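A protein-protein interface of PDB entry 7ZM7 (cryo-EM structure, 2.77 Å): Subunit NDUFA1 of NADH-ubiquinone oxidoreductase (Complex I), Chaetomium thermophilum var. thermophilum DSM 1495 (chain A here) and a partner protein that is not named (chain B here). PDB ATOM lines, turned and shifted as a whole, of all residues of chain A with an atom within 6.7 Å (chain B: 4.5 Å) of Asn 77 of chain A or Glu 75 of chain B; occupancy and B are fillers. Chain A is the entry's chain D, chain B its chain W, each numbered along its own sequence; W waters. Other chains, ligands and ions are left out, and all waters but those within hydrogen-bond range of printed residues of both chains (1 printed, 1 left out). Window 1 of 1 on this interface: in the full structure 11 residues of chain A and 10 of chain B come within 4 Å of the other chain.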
ATOM      1  N   ARG A  55      29.625   2.553 -12.854  1.00  0.00           N
ATOM      2  CA  ARG A  55      29.663   3.728 -13.706  1.00  0.00           C
ATOM      3  C   ARG A  55      30.708   4.722 -13.234  1.00  0.00           C
ATOM      4  O   ARG A  55      31.389   5.345 -14.050  1.00  0.00           O
ATOM      5  CB  ARG A  55      28.290   4.387 -13.747  1.00  0.00           C
ATOM      6  CG  ARG A  55      27.342   3.740 -14.692  1.00  0.00           C
ATOM      7  CD  ARG A  55      25.995   4.368 -14.597  1.00  0.00           C
ATOM      8  NE  ARG A  55      25.976   5.663 -15.243  1.00  0.00           N
ATOM      9  CZ  ARG A  55      25.335   6.722 -14.776  1.00  0.00           C
ATOM     10  NH1 ARG A  55      24.665   6.641 -13.644  1.00  0.00           N
ATOM     11  NH2 ARG A  55      25.372   7.862 -15.441  1.00  0.00           N
ATOM     12  N   GLY A  72      32.014  12.477 -18.762  1.00  0.00           N
ATOM     13  CA  GLY A  72      31.572  11.247 -19.368  1.00  0.00           C
ATOM     14  C   GLY A  72      30.569  10.467 -18.549  1.00  0.00           C
ATOM     15  O   GLY A  72      29.853   9.639 -19.111  1.00  0.00           O
ATOM     16  N   PHE A  73      30.472  10.719 -17.240  1.00  0.00           N
ATOM     17  CA  PHE A  73      29.539   9.963 -16.358  1.00  0.00           C
ATOM     18  C   PHE A  73      28.115  10.031 -16.910  1.00  0.00           C
ATOM     19  O   PHE A  73      27.382   9.041 -16.829  1.00  0.00           O
ATOM     20  CB  PHE A  73      29.536  10.539 -14.941  1.00  0.00           C
ATOM     21  CG  PHE A  73      28.572   9.875 -13.994  1.00  0.00           C
ATOM     22  CD1 PHE A  73      28.735   8.548 -13.635  1.00  0.00           C
ATOM     23  CD2 PHE A  73      27.495  10.571 -13.471  1.00  0.00           C
ATOM     24  CE1 PHE A  73      27.843   7.935 -12.773  1.00  0.00           C
ATOM     25  CE2 PHE A  73      26.612   9.959 -12.599  1.00  0.00           C
ATOM     26  CZ  PHE A  73      26.788   8.642 -12.250  1.00  0.00           C
ATOM     27  N   GLU A  74      27.744  11.169 -17.495  1.00  0.00           N
ATOM     28  CA  GLU A  74      26.371  11.365 -18.015  1.00  0.00           C
ATOM     29  C   GLU A  74      26.013  10.323 -19.097  1.00  0.00           C
ATOM     30  O   GLU A  74      24.827   9.975 -19.178  1.00  0.00           O
ATOM     31  CB  GLU A  74      26.275  12.793 -18.532  1.00  0.00           C
ATOM     32  CG  GLU A  74      27.518  13.256 -19.271  1.00  0.00           C
ATOM     33  CD  GLU A  74      28.480  14.120 -18.474  1.00  0.00           C
ATOM     34  OE1 GLU A  74      29.161  13.583 -17.577  1.00  0.00           O
ATOM     35  OE2 GLU A  74      28.545  15.333 -18.750  1.00  0.00           O
ATOM     36  N   PHE A  75      26.964   9.876 -19.922  1.00  0.00           N
ATOM     37  CA  PHE A  75      26.669   8.952 -21.049  1.00  0.00           C
ATOM     38  C   PHE A  75      26.944   7.471 -20.744  1.00  0.00           C
ATOM     39  O   PHE A  75      26.637   6.656 -21.621  1.00  0.00           O
ATOM     40  CB  PHE A  75      27.565   9.317 -22.236  1.00  0.00           C
ATOM     41  CG  PHE A  75      27.595  10.785 -22.568  1.00  0.00           C
ATOM     42  CD1 PHE A  75      26.489  11.406 -23.120  1.00  0.00           C
ATOM     43  CD2 PHE A  75      28.730  11.541 -22.328  1.00  0.00           C
ATOM     44  CE1 PHE A  75      26.514  12.757 -23.419  1.00  0.00           C
ATOM     45  CE2 PHE A  75      28.751  12.893 -22.630  1.00  0.00           C
ATOM     46  CZ  PHE A  75      27.644  13.498 -23.173  1.00  0.00           C
ATOM     47  N   ASN A  76      27.480   7.117 -19.573  1.00  0.00           N
ATOM     48  CA  ASN A  76      27.876   5.710 -19.289  1.00  0.00           C
ATOM     49  C   ASN A  76      26.731   4.942 -18.635  1.00  0.00           C
ATOM     50  O   ASN A  76      26.948   3.773 -18.290  1.00  0.00           O
ATOM     51  CB  ASN A  76      29.202   5.602 -18.535  1.00  0.00           C
ATOM     52  CG  ASN A  76      29.240   6.250 -17.170  1.00  0.00           C
ATOM     53  OD1 ASN A  76      28.209   6.498 -16.559  1.00  0.00           O
ATOM     54  ND2 ASN A  76      30.436   6.501 -16.669  1.00  0.00           N
ATOM     55  N   ASN A  77      25.566   5.573 -18.493  1.00  0.00           N
ATOM     56  CA  ASN A  77      24.369   4.939 -17.879  1.00  0.00           C
ATOM     57  C   ASN A  77      24.014   3.736 -18.740  1.00  0.00           C
ATOM     58  O   ASN A  77      23.679   3.948 -19.911  1.00  0.00           O
ATOM     59  CB  ASN A  77      23.212   5.926 -17.724  1.00  0.00           C
ATOM     60  CG  ASN A  77      22.030   5.331 -16.990  1.00  0.00           C
ATOM     61  OD1 ASN A  77      22.203   4.532 -16.075  1.00  0.00           O
ATOM     62  ND2 ASN A  77      20.828   5.716 -17.379  1.00  0.00           N
ATOM     63  N   PRO A  78      24.020   2.499 -18.217  1.00  0.00           N
ATOM     64  CA  PRO A  78      23.821   1.324 -19.058  1.00  0.00           C
ATOM     65  C   PRO A  78      22.351   0.961 -19.284  1.00  0.00           C
ATOM     66  O   PRO A  78      21.646   0.757 -18.327  1.00  0.00           O
ATOM     67  CB  PRO A  78      24.547   0.233 -18.268  1.00  0.00           C
ATOM     68  CG  PRO A  78      24.487   0.672 -16.813  1.00  0.00           C
ATOM     69  CD  PRO A  78      24.216   2.163 -16.810  1.00  0.00           C
ATOM     70  N   TRP A  79      21.898   0.960 -20.535  1.00  0.00           N
ATOM     71  CA  TRP A  79      20.524   0.474 -20.815  1.00  0.00           C
ATOM     72  C   TRP A  79      20.675  -0.940 -21.364  1.00  0.00           C
ATOM     73  O   TRP A  79      21.262  -1.091 -22.435  1.00  0.00           O
ATOM     74  CB  TRP A  79      19.757   1.400 -21.767  1.00  0.00           C
ATOM     75  CG  TRP A  79      19.230   2.667 -21.166  1.00  0.00           C
ATOM     76  CD1 TRP A  79      19.620   3.255 -20.000  1.00  0.00           C
ATOM     77  CD2 TRP A  79      18.215   3.519 -21.725  1.00  0.00           C
ATOM     78  NE1 TRP A  79      18.913   4.407 -19.792  1.00  0.00           N
ATOM     79  CE2 TRP A  79      18.044   4.595 -20.833  1.00  0.00           C
ATOM     80  CE3 TRP A  79      17.441   3.480 -22.889  1.00  0.00           C
ATOM     81  CZ2 TRP A  79      17.126   5.617 -21.066  1.00  0.00           C
ATOM     82  CZ3 TRP A  79      16.536   4.492 -23.122  1.00  0.00           C
ATOM     83  CH2 TRP A  79      16.381   5.543 -22.220  1.00  0.00           C
ATOM     84  N   LEU B  71      18.680  10.497  -7.197  1.00  0.00           N
ATOM     85  CA  LEU B  71      18.921   9.377  -8.137  1.00  0.00           C
ATOM     86  C   LEU B  71      17.936   9.441  -9.298  1.00  0.00           C
ATOM     87  O   LEU B  71      18.349   9.125 -10.418  1.00  0.00           O
ATOM     88  CB  LEU B  71      18.885   8.042  -7.388  1.00  0.00           C
ATOM     89  CG  LEU B  71      20.060   7.784  -6.450  1.00  0.00           C
ATOM     90  CD1 LEU B  71      19.685   6.775  -5.383  1.00  0.00           C
ATOM     91  CD2 LEU B  71      21.275   7.321  -7.229  1.00  0.00           C
ATOM     92  N   GLN B  72      16.679   9.781  -9.024  1.00  0.00           N
ATOM     93  CA  GLN B  72      15.622   9.891 -10.050  1.00  0.00           C
ATOM     94  C   GLN B  72      15.925  11.052 -10.988  1.00  0.00           C
ATOM     95  O   GLN B  72      15.693  10.906 -12.184  1.00  0.00           O
ATOM     96  CB  GLN B  72      14.273  10.024  -9.348  1.00  0.00           C
ATOM     97  CG  GLN B  72      13.079   9.906 -10.280  1.00  0.00           C
ATOM     98  CD  GLN B  72      13.016   8.553 -10.940  1.00  0.00           C
ATOM     99  OE1 GLN B  72      13.313   7.525 -10.338  1.00  0.00           O
ATOM    100  NE2 GLN B  72      12.611   8.544 -12.197  1.00  0.00           N
ATOM    101  N   ALA B  73      16.429  12.149 -10.451  1.00  0.00           N
ATOM    102  CA  ALA B  73      16.703  13.361 -11.246  1.00  0.00           C
ATOM    103  C   ALA B  73      17.769  13.060 -12.287  1.00  0.00           C
ATOM    104  O   ALA B  73      17.629  13.537 -13.422  1.00  0.00           O
ATOM    105  CB  ALA B  73      17.103  14.472 -10.311  1.00  0.00           C
ATOM    106  N   GLU B  74      18.787  12.297 -11.905  1.00  0.00           N
ATOM    107  CA  GLU B  74      19.847  11.905 -12.853  1.00  0.00           C
ATOM    108  C   GLU B  74      19.247  11.030 -13.952  1.00  0.00           C
ATOM    109  O   GLU B  74      19.594  11.251 -15.118  1.00  0.00           O
ATOM    110  CB  GLU B  74      20.920  11.168 -12.068  1.00  0.00           C
ATOM    111  CG  GLU B  74      22.173  10.920 -12.875  1.00  0.00           C
ATOM    112  CD  GLU B  74      22.906   9.647 -12.507  1.00  0.00           C
ATOM    113  OE1 GLU B  74      22.881   9.269 -11.320  1.00  0.00           O
ATOM    114  OE2 GLU B  74      23.482   9.034 -13.415  1.00  0.00           O
ATOM    115  N   GLU B  75      18.390  10.084 -13.592  1.00  0.00           N
ATOM    116  CA  GLU B  75      17.745   9.176 -14.560  1.00  0.00           C
ATOM    117  C   GLU B  75      16.841   9.968 -15.497  1.00  0.00           C
ATOM    118  O   GLU B  75      16.846   9.671 -16.691  1.00  0.00           O
ATOM    119  CB  GLU B  75      16.913   8.189 -13.771  1.00  0.00           C
ATOM    120  CG  GLU B  75      16.520   6.948 -14.539  1.00  0.00           C
ATOM    121  CD  GLU B  75      17.628   5.923 -14.656  1.00  0.00           C
ATOM    122  OE1 GLU B  75      18.556   5.965 -13.823  1.00  0.00           O
ATOM    123  OE2 GLU B  75      17.566   5.099 -15.585  1.00  0.00           O
ATOM    124  N   ASP B  76      16.119  10.948 -14.965  1.00  0.00           N
ATOM    125  CA  ASP B  76      15.170  11.763 -15.756  1.00  0.00           C
ATOM    126  C   ASP B  76      15.912  12.579 -16.816  1.00  0.00           C
ATOM    127  O   ASP B  76      15.406  12.668 -17.937  1.00  0.00           O
ATOM    128  CB  ASP B  76      14.288  12.581 -14.817  1.00  0.00           C
ATOM    129  CG  ASP B  76      13.253  11.730 -14.111  1.00  0.00           C
ATOM    130  OD1 ASP B  76      13.290  10.504 -14.298  1.00  0.00           O
ATOM    131  OD2 ASP B  76      12.411  12.299 -13.391  1.00  0.00           O
ATOM    132  N   ARG B  77      17.068  13.149 -16.468  1.00  0.00           N
ATOM    133  CA  ARG B  77      17.888  13.904 -17.455  1.00  0.00           C
ATOM    134  C   ARG B  77      18.339  12.943 -18.558  1.00  0.00           C
ATOM    135  O   ARG B  77      18.324  13.346 -19.724  1.00  0.00           O
ATOM    136  CB  ARG B  77      19.035  14.650 -16.765  1.00  0.00           C
ATOM    137  CG  ARG B  77      18.597  15.902 -16.022  1.00  0.00           C
ATOM    138  CD  ARG B  77      19.767  16.606 -15.368  1.00  0.00           C
ATOM    139  NE  ARG B  77      19.486  16.885 -13.969  1.00  0.00           N
ATOM    140  CZ  ARG B  77      19.945  16.165 -12.957  1.00  0.00           C
ATOM    141  NH1 ARG B  77      20.731  15.128 -13.187  1.00  0.00           N
ATOM    142  NH2 ARG B  77      19.632  16.491 -11.717  1.00  0.00           N
ATOM    143  N   ASP B  78      18.716  11.719 -18.187  1.00  0.00           N
ATOM    144  CA  ASP B  78      19.153  10.678 -19.153  1.00  0.00           C
ATOM    145  C   ASP B  78      17.972  10.224 -20.024  1.00  0.00           C
ATOM    146  O   ASP B  78      18.199   9.947 -21.195  1.00  0.00           O
ATOM    147  CB  ASP B  78      19.856   9.554 -18.397  1.00  0.00           C
ATOM    148  CG  ASP B  78      20.702   8.643 -19.265  1.00  0.00           C
ATOM    149  OD1 ASP B  78      21.815   9.064 -19.629  1.00  0.00           O
ATOM    150  OD2 ASP B  78      20.250   7.520 -19.552  1.00  0.00           O
ATOM    151  N   HIS B  79      16.774  10.105 -19.453  1.00  0.00           N
ATOM    152  CA  HIS B  79      15.544   9.754 -20.209  1.00  0.00           C
ATOM    153  C   HIS B  79      15.175  10.870 -21.183  1.00  0.00           C
ATOM    154  O   HIS B  79      14.594  10.573 -22.224  1.00  0.00           O
ATOM    155  CB  HIS B  79      14.399   9.352 -19.270  1.00  0.00           C
ATOM    156  CG  HIS B  79      14.501   7.941 -18.807  1.00  0.00           C
ATOM    157  ND1 HIS B  79      13.888   6.905 -19.474  1.00  0.00           N
ATOM    158  CD2 HIS B  79      15.163   7.386 -17.775  1.00  0.00           C
ATOM    159  CE1 HIS B  79      14.152   5.776 -18.860  1.00  0.00           C
ATOM    160  NE2 HIS B  79      14.937   6.043 -17.819  1.00  0.00           N
ATOM    161  N   ARG B  82      18.126  10.727 -24.100  1.00  0.00           N
ATOM    162  CA  ARG B  82      18.015   9.675 -25.098  1.00  0.00           C
ATOM    163  C   ARG B  82      16.725   9.777 -25.886  1.00  0.00           C
ATOM    164  O   ARG B  82      16.672   9.327 -27.031  1.00  0.00           O
ATOM    165  CB  ARG B  82      18.133   8.308 -24.439  1.00  0.00           C
ATOM    166  CG  ARG B  82      19.435   8.113 -23.715  1.00  0.00           C
ATOM    167  CD  ARG B  82      19.601   6.711 -23.246  1.00  0.00           C
ATOM    168  NE  ARG B  82      19.652   5.760 -24.341  1.00  0.00           N
ATOM    169  CZ  ARG B  82      20.504   4.754 -24.389  1.00  0.00           C
ATOM    170  NH1 ARG B  82      20.502   3.928 -25.411  1.00  0.00           N
ATOM    171  NH2 ARG B  82      21.361   4.585 -23.405  1.00  0.00           N
HETATM  172  O   HOH W   1      21.030   7.939 -15.105  1.00  0.00           O
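Of the 10 printed residues of chain B, 5 touch a printed residue of chain A.
Printed residues of chain B that touch a printed residue of chain A: Glu 74, Glu 75, Asp 78, His 79 and Arg 82.
Hydrophobic or aromatic side chains of chain B within 4 Å of the printed part of chain A: His 79.
Along chain B the printed residues that touch a printed residue of chain A span positions 74 to 82.
Of the 9 printed residues of chain A, 5 touch a printed residue of chain B.
Water W1 lies within hydrogen-bond range of the side-chain carboxylate of Glu 74 of chain B (3.2 Å), the side-chain amide nitrogen of Asn 77 of chain A (3.2 Å) and the side-chain carboxylate of Glu 75 of chain B (3.4 Å).
Among the printed residues, merely in contact across the chains: Phe 73 of chain A with Glu 74 of chain B, Asn 77 of chain A with Glu 75 of chain B, Trp 79 of chain A with His 79 of chain B and Trp 79 of chain A with Arg 82 of chain B.
The backbone carbonyl oxygen of Phe 73 of chain A lies within hydrogen-bond range of the guanidinium group of Arg 55 of chain A (2.7 Å).
The guanidinium group of Arg 55 of chain A is in hydrogen-bond range of the side-chain amide oxygen of Asn 76 of chain A (2.7 Å).
The backbone NH (N) of Gly 72 of chain A sits at hydrogen-bond distance from the side-chain carboxylate (OE1) of Glu 74 of chain A, 3.3 Å away.
O of Phe 73 of chain A sits close to OD1 of Asn 76 of chain A.
ND2 of Asn 77 of chain A sits close to NE1 of Trp 79 of chain A (3.3 Å).
Printed residues of chain B within 4 Å of Arg 55 of chain A: Glu 74.
Printed residues of chain B within 4 Å of Phe 73 of chain A: Glu 74 (3.4 Å).
Asn 77 of chain A touches just these residues of chain B: Glu 75 (3.8 Å) and Asp 78 (2.9 Å).
Of the printed residues of chain B, Trp 79 of chain A touches Asp 78, His 79 and Arg 82.
Printed residues of chain A within 4 Å of Glu 74 of chain B: Arg 55 and Phe 73.
Printed residues of chain A within 4 Å of Glu 75 of chain B: Asn 77.
Of the printed residues of chain A, Asp 78 of chain B touches Glu 74, Asn 77 and Trp 79.
The nearest residue of chain B that does not touch Asn 77 of chain A is Arg 82 of chain B (4.2 Å).
The nearest residue of chain A that does not touch Glu 75 of chain B is Trp 79 of chain A (4.5 Å).
The nearest printed residue of chain A that does not touch Glu 74 of chain B is Asn 77 of chain A (5.3 Å).
The side-chain carboxylate (OE2) of Glu 74 of chain B lies within salt-bridge range of the guanidinium group (NH1) of Arg 55 of chain A.
The side-chain amide nitrogen (ND2) of Asn 77 of chain A sits at hydrogen-bond distance from the side-chain carboxylate (OD2) of Asp 78 of chain B, 2.9 Å away.
The side-chain carboxylate of Asp 78 of chain B is in hydrogen-bond range of the indole nitrogen of Trp 79 of chain A, at 3.4 Å.
The backbone carbonyl oxygen (O) of Glu 74 of chain A lies close to the side-chain carboxylate (OD1) of Asp 78 of chain B (3.2 Å).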
